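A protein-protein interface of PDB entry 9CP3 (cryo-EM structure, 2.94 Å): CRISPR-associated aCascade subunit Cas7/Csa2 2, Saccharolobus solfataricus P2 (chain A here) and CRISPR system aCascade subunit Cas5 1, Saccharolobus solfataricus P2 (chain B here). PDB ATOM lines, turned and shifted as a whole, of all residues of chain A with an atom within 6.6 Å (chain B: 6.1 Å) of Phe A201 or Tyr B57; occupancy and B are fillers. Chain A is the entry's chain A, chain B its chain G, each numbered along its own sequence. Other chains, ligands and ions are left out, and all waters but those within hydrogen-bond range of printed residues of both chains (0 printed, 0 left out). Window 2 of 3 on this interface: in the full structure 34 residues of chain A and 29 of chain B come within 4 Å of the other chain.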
ATOM      1  N   TYR A 101       7.096 -24.458  -0.646  1.00  0.00           N
ATOM      2  CA  TYR A 101       8.129 -23.932   0.240  1.00  0.00           C
ATOM      3  C   TYR A 101       9.522 -24.312  -0.243  1.00  0.00           C
ATOM      4  O   TYR A 101      10.428 -23.471  -0.264  1.00  0.00           O
ATOM      5  CB  TYR A 101       7.900 -24.437   1.664  1.00  0.00           C
ATOM      6  CG  TYR A 101       6.528 -24.123   2.215  1.00  0.00           C
ATOM      7  CD1 TYR A 101       6.211 -22.845   2.655  1.00  0.00           C
ATOM      8  CD2 TYR A 101       5.549 -25.105   2.293  1.00  0.00           C
ATOM      9  CE1 TYR A 101       4.958 -22.554   3.159  1.00  0.00           C
ATOM     10  CE2 TYR A 101       4.293 -24.823   2.795  1.00  0.00           C
ATOM     11  CZ  TYR A 101       4.002 -23.547   3.227  1.00  0.00           C
ATOM     12  OH  TYR A 101       2.753 -23.263   3.727  1.00  0.00           O
ATOM     13  N   ASN A 102       9.710 -25.572  -0.647  1.00  0.00           N
ATOM     14  CA  ASN A 102      11.037 -26.043  -1.033  1.00  0.00           C
ATOM     15  C   ASN A 102      11.574 -25.294  -2.245  1.00  0.00           C
ATOM     16  O   ASN A 102      12.791 -25.115  -2.374  1.00  0.00           O
ATOM     17  CB  ASN A 102      11.000 -27.544  -1.314  1.00  0.00           C
ATOM     18  CG  ASN A 102      10.933 -28.371  -0.046  1.00  0.00           C
ATOM     19  OD1 ASN A 102      11.944 -28.892   0.423  1.00  0.00           O
ATOM     20  ND2 ASN A 102       9.737 -28.493   0.519  1.00  0.00           N
ATOM     21  N   ALA A 104      10.779 -22.148  -2.838  1.00  0.00           N
ATOM     22  CA  ALA A 104      10.686 -20.716  -2.565  1.00  0.00           C
ATOM     23  C   ALA A 104      11.994 -20.009  -2.889  1.00  0.00           C
ATOM     24  O   ALA A 104      11.991 -18.926  -3.488  1.00  0.00           O
ATOM     25  CB  ALA A 104      10.294 -20.484  -1.107  1.00  0.00           C
ATOM     26  N   ARG A 105      13.122 -20.612  -2.507  1.00  0.00           N
ATOM     27  CA  ARG A 105      14.425 -20.054  -2.852  1.00  0.00           C
ATOM     28  C   ARG A 105      14.526 -19.813  -4.353  1.00  0.00           C
ATOM     29  O   ARG A 105      14.955 -18.740  -4.795  1.00  0.00           O
ATOM     30  CB  ARG A 105      15.538 -20.988  -2.375  1.00  0.00           C
ATOM     31  CG  ARG A 105      16.932 -20.404  -2.503  1.00  0.00           C
ATOM     32  CD  ARG A 105      17.893 -21.061  -1.529  1.00  0.00           C
ATOM     33  NE  ARG A 105      19.218 -20.455  -1.579  1.00  0.00           N
ATOM     34  CZ  ARG A 105      20.096 -20.494  -0.587  1.00  0.00           C
ATOM     35  NH1 ARG A 105      19.825 -21.110   0.553  1.00  0.00           N
ATOM     36  NH2 ARG A 105      21.275 -19.899  -0.740  1.00  0.00           N
ATOM     37  N   PRO A 198      20.865 -14.877  -1.154  1.00  0.00           N
ATOM     38  CA  PRO A 198      19.488 -15.312  -0.894  1.00  0.00           C
ATOM     39  C   PRO A 198      19.253 -15.508   0.596  1.00  0.00           C
ATOM     40  O   PRO A 198      20.127 -15.982   1.325  1.00  0.00           O
ATOM     41  CB  PRO A 198      19.381 -16.635  -1.662  1.00  0.00           C
ATOM     42  CG  PRO A 198      20.473 -16.584  -2.678  1.00  0.00           C
ATOM     43  CD  PRO A 198      21.578 -15.783  -2.069  1.00  0.00           C
ATOM     44  N   SER A 199      18.057 -15.133   1.049  1.00  0.00           N
ATOM     45  CA  SER A 199      17.742 -15.108   2.471  1.00  0.00           C
ATOM     46  C   SER A 199      16.746 -16.188   2.874  1.00  0.00           C
ATOM     47  O   SER A 199      16.136 -16.094   3.944  1.00  0.00           O
ATOM     48  CB  SER A 199      17.213 -13.730   2.869  1.00  0.00           C
ATOM     49  OG  SER A 199      17.050 -13.639   4.273  1.00  0.00           O
ATOM     50  N   THR A 200      16.567 -17.213   2.046  1.00  0.00           N
ATOM     51  CA  THR A 200      15.702 -18.339   2.365  1.00  0.00           C
ATOM     52  C   THR A 200      16.549 -19.598   2.470  1.00  0.00           C
ATOM     53  O   THR A 200      17.282 -19.937   1.535  1.00  0.00           O
ATOM     54  CB  THR A 200      14.610 -18.520   1.307  1.00  0.00           C
ATOM     55  OG1 THR A 200      13.955 -17.267   1.076  1.00  0.00           O
ATOM     56  CG2 THR A 200      13.585 -19.542   1.773  1.00  0.00           C
ATOM     57  N   PHE A 201      16.447 -20.285   3.604  1.00  0.00           N
ATOM     58  CA  PHE A 201      17.263 -21.468   3.832  1.00  0.00           C
ATOM     59  C   PHE A 201      16.822 -22.605   2.918  1.00  0.00           C
ATOM     60  O   PHE A 201      15.631 -22.787   2.654  1.00  0.00           O
ATOM     61  CB  PHE A 201      17.176 -21.902   5.295  1.00  0.00           C
ATOM     62  CG  PHE A 201      18.398 -22.624   5.783  1.00  0.00           C
ATOM     63  CD1 PHE A 201      19.538 -21.921   6.136  1.00  0.00           C
ATOM     64  CD2 PHE A 201      18.409 -24.004   5.888  1.00  0.00           C
ATOM     65  CE1 PHE A 201      20.665 -22.579   6.586  1.00  0.00           C
ATOM     66  CE2 PHE A 201      19.533 -24.669   6.338  1.00  0.00           C
ATOM     67  CZ  PHE A 201      20.663 -23.956   6.687  1.00  0.00           C
ATOM     68  N   GLY A 202      17.792 -23.372   2.436  1.00  0.00           N
ATOM     69  CA  GLY A 202      17.498 -24.482   1.552  1.00  0.00           C
ATOM     70  C   GLY A 202      18.733 -24.863   0.753  1.00  0.00           C
ATOM     71  O   GLY A 202      19.851 -24.480   1.091  1.00  0.00           O
ATOM     72  N   GLU A 203      18.496 -25.625  -0.310  1.00  0.00           N
ATOM     73  CA  GLU A 203      19.561 -26.061  -1.198  1.00  0.00           C
ATOM     74  C   GLU A 203      19.760 -25.054  -2.322  1.00  0.00           C
ATOM     75  O   GLU A 203      18.819 -24.383  -2.757  1.00  0.00           O
ATOM     76  CB  GLU A 203      19.249 -27.439  -1.784  1.00  0.00           C
ATOM     77  CG  GLU A 203      18.818 -28.468  -0.754  1.00  0.00           C
ATOM     78  CD  GLU A 203      18.637 -29.849  -1.352  1.00  0.00           C
ATOM     79  OE1 GLU A 203      18.809 -29.993  -2.581  1.00  0.00           O
ATOM     80  OE2 GLU A 203      18.323 -30.790  -0.594  1.00  0.00           O
ATOM     81  N   VAL B  48      19.574 -14.791   7.809  1.00  0.00           N
ATOM     82  CA  VAL B  48      18.472 -15.699   7.518  1.00  0.00           C
ATOM     83  C   VAL B  48      17.180 -15.018   7.948  1.00  0.00           C
ATOM     84  O   VAL B  48      16.964 -14.768   9.138  1.00  0.00           O
ATOM     85  CB  VAL B  48      18.649 -17.051   8.221  1.00  0.00           C
ATOM     86  CG1 VAL B  48      17.442 -17.941   7.966  1.00  0.00           C
ATOM     87  CG2 VAL B  48      19.926 -17.727   7.750  1.00  0.00           C
ATOM     88  N   ASN B  50      14.286 -16.500   6.990  1.00  0.00           N
ATOM     89  CA  ASN B  50      13.329 -17.603   7.015  1.00  0.00           C
ATOM     90  C   ASN B  50      14.107 -18.907   7.040  1.00  0.00           C
ATOM     91  O   ASN B  50      14.907 -19.166   6.135  1.00  0.00           O
ATOM     92  CB  ASN B  50      12.395 -17.546   5.805  1.00  0.00           C
ATOM     93  CG  ASN B  50      11.049 -18.189   6.075  1.00  0.00           C
ATOM     94  OD1 ASN B  50      10.747 -18.570   7.205  1.00  0.00           O
ATOM     95  ND2 ASN B  50      10.230 -18.309   5.037  1.00  0.00           N
ATOM     96  N   ILE B  51      13.880 -19.719   8.069  1.00  0.00           N
ATOM     97  CA  ILE B  51      14.493 -21.035   8.196  1.00  0.00           C
ATOM     98  C   ILE B  51      13.399 -22.042   8.516  1.00  0.00           C
ATOM     99  O   ILE B  51      12.454 -21.736   9.252  1.00  0.00           O
ATOM    100  CB  ILE B  51      15.601 -21.055   9.273  1.00  0.00           C
ATOM    101  CG1 ILE B  51      16.379 -22.372   9.220  1.00  0.00           C
ATOM    102  CG2 ILE B  51      15.026 -20.816  10.662  1.00  0.00           C
ATOM    103  CD1 ILE B  51      17.465 -22.483  10.267  1.00  0.00           C
ATOM    104  N   ASN B  52      13.508 -23.236   7.939  1.00  0.00           N
ATOM    105  CA  ASN B  52      12.471 -24.241   8.123  1.00  0.00           C
ATOM    106  C   ASN B  52      12.481 -24.752   9.558  1.00  0.00           C
ATOM    107  O   ASN B  52      13.514 -25.202  10.063  1.00  0.00           O
ATOM    108  CB  ASN B  52      12.672 -25.398   7.148  1.00  0.00           C
ATOM    109  CG  ASN B  52      11.422 -26.238   6.980  1.00  0.00           C
ATOM    110  OD1 ASN B  52      10.305 -25.749   7.154  1.00  0.00           O
ATOM    111  ND2 ASN B  52      11.602 -27.509   6.643  1.00  0.00           N
ATOM    112  N   LEU B  53      11.325 -24.679  10.214  1.00  0.00           N
ATOM    113  CA  LEU B  53      11.151 -25.187  11.566  1.00  0.00           C
ATOM    114  C   LEU B  53      10.456 -26.540  11.593  1.00  0.00           C
ATOM    115  O   LEU B  53      10.110 -27.029  12.672  1.00  0.00           O
ATOM    116  CB  LEU B  53      10.366 -24.182  12.409  1.00  0.00           C
ATOM    117  CG  LEU B  53      10.845 -22.732  12.332  1.00  0.00           C
ATOM    118  CD1 LEU B  53       9.834 -21.807  12.982  1.00  0.00           C
ATOM    119  CD2 LEU B  53      12.209 -22.585  12.985  1.00  0.00           C
ATOM    120  N   TYR B  57       7.308 -23.143   7.657  1.00  0.00           N
ATOM    121  CA  TYR B  57       8.348 -22.155   7.891  1.00  0.00           C
ATOM    122  C   TYR B  57       7.910 -21.156   8.959  1.00  0.00           C
ATOM    123  O   TYR B  57       6.727 -21.029   9.287  1.00  0.00           O
ATOM    124  CB  TYR B  57       8.690 -21.415   6.597  1.00  0.00           C
ATOM    125  CG  TYR B  57       9.705 -22.119   5.728  1.00  0.00           C
ATOM    126  CD1 TYR B  57       9.358 -23.238   4.986  1.00  0.00           C
ATOM    127  CD2 TYR B  57      11.010 -21.655   5.640  1.00  0.00           C
ATOM    128  CE1 TYR B  57      10.284 -23.881   4.186  1.00  0.00           C
ATOM    129  CE2 TYR B  57      11.942 -22.290   4.843  1.00  0.00           C
ATOM    130  CZ  TYR B  57      11.575 -23.402   4.118  1.00  0.00           C
ATOM    131  OH  TYR B  57      12.501 -24.038   3.323  1.00  0.00           O
ATOM    132  N   GLY B  58       8.886 -20.441   9.500  1.00  0.00           N
ATOM    133  CA  GLY B  58       8.600 -19.453  10.520  1.00  0.00           C
ATOM    134  C   GLY B  58       9.799 -18.569  10.767  1.00  0.00           C
ATOM    135  O   GLY B  58      10.807 -18.641  10.062  1.00  0.00           O
ATOM    136  N   SER B  59       9.673 -17.722  11.783  1.00  0.00           N
ATOM    137  CA  SER B  59      10.746 -16.794  12.105  1.00  0.00           C
ATOM    138  C   SER B  59      11.968 -17.558  12.614  1.00  0.00           C
ATOM    139  O   SER B  59      11.823 -18.580  13.292  1.00  0.00           O
ATOM    140  CB  SER B  59      10.281 -15.783  13.152  1.00  0.00           C
ATOM    141  OG  SER B  59      11.359 -14.985  13.609  1.00  0.00           O
ATOM    142  N   ILE B 198       5.948 -18.444  14.509  1.00  0.00           N
ATOM    143  CA  ILE B 198       5.611 -19.008  13.208  1.00  0.00           C
ATOM    144  C   ILE B 198       4.543 -18.140  12.558  1.00  0.00           C
ATOM    145  O   ILE B 198       3.422 -18.027  13.064  1.00  0.00           O
ATOM    146  CB  ILE B 198       5.135 -20.459  13.346  1.00  0.00           C
ATOM    147  CG1 ILE B 198       6.251 -21.336  13.917  1.00  0.00           C
ATOM    148  CG2 ILE B 198       4.660 -20.993  12.004  1.00  0.00           C
ATOM    149  CD1 ILE B 198       5.785 -22.706  14.352  1.00  0.00           C
ATOM    150  N   TRP B 199       4.892 -17.522  11.431  1.00  0.00           N
ATOM    151  CA  TRP B 199       3.948 -16.681  10.710  1.00  0.00           C
ATOM    152  C   TRP B 199       2.789 -17.514  10.174  1.00  0.00           C
ATOM    153  O   TRP B 199       2.920 -18.713   9.913  1.00  0.00           O
ATOM    154  CB  TRP B 199       4.654 -15.940   9.573  1.00  0.00           C
ATOM    155  CG  TRP B 199       5.393 -16.836   8.626  1.00  0.00           C
ATOM    156  CD1 TRP B 199       6.734 -17.083   8.618  1.00  0.00           C
ATOM    157  CD2 TRP B 199       4.840 -17.591   7.540  1.00  0.00           C
ATOM    158  NE1 TRP B 199       7.051 -17.950   7.602  1.00  0.00           N
ATOM    159  CE2 TRP B 199       5.906 -18.277   6.925  1.00  0.00           C
ATOM    160  CE3 TRP B 199       3.549 -17.756   7.030  1.00  0.00           C
ATOM    161  CZ2 TRP B 199       5.720 -19.114   5.828  1.00  0.00           C
ATOM    162  CZ3 TRP B 199       3.366 -18.590   5.943  1.00  0.00           C
ATOM    163  CH2 TRP B 199       4.446 -19.257   5.352  1.00  0.00           C
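Printed residues of chain B within 4 Å of Phe A201: Asn B50, Ile B51 and Tyr B57.
Of chain A, only Tyr A101 and Phe A201 come within 4 Å of Tyr B57.
Of the printed residues of chain A, Trp B199 touches Tyr A101.
Printed residues of chain B within 4 Å of Ser A199: Val B48 (3.9 Å) and Asn B50 (3.6 Å).
Of the printed residues of chain A, Asn B50 touches Ser A199, Thr A200 and Phe A201.
Of the printed residues of chain A, Ile B51 touches Phe A201 (3.99 Å).
Ala A104 touches none of the printed residues of chain B.
The nearest printed residue of chain B that does not touch Phe A201 is Val B48 (4.5 Å).
The nearest printed residue of chain B that does not touch Thr A200 is Tyr B57 (4.4 Å).
The backbone NH (N) of Phe A201 sits at hydrogen-bond distance from the backbone carbonyl oxygen (O) of Asn B50.
OH of Tyr B57 sits at hydrogen-bond distance from O of Phe A201 (3.4 Å).
The guanidinium group (NH1) of Arg A105 lies within hydrogen-bond range of the backbone carbonyl oxygen (O) of Thr A200 (3.0 Å).
The backbone carbonyl oxygen (O) of Gly B58 lies close to the side-chain amide oxygen (OD1) of Asn B50 (2.9 Å).
CB of Tyr A101 touches CE1 of Tyr B57 (3.5 Å).
Trp B199 touches Tyr A101.
OG of Ser A199 touches C of Val B48, at 3.9 Å.
Asn B50 touches Ser A199 (N to O, 3.6 Å).
Thr A200 touches Asn B50.
Ile B51 touches Phe A201.
Of the 10 printed residues of chain B, 5 touch a printed residue of chain A.
Hydrophobic or aromatic side chains of chain B that line the printed part of chain A: Ile B51, Tyr B57 and Trp B199.
Printed residues of chain A that touch a printed residue of chain B: Tyr A101, Ser A199, Thr A200 and Phe A201.
Among the printed residues, no Asp or Glu carboxylate lies within 4 Å of a Lys or Arg side-chain nitrogen of the other chain.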
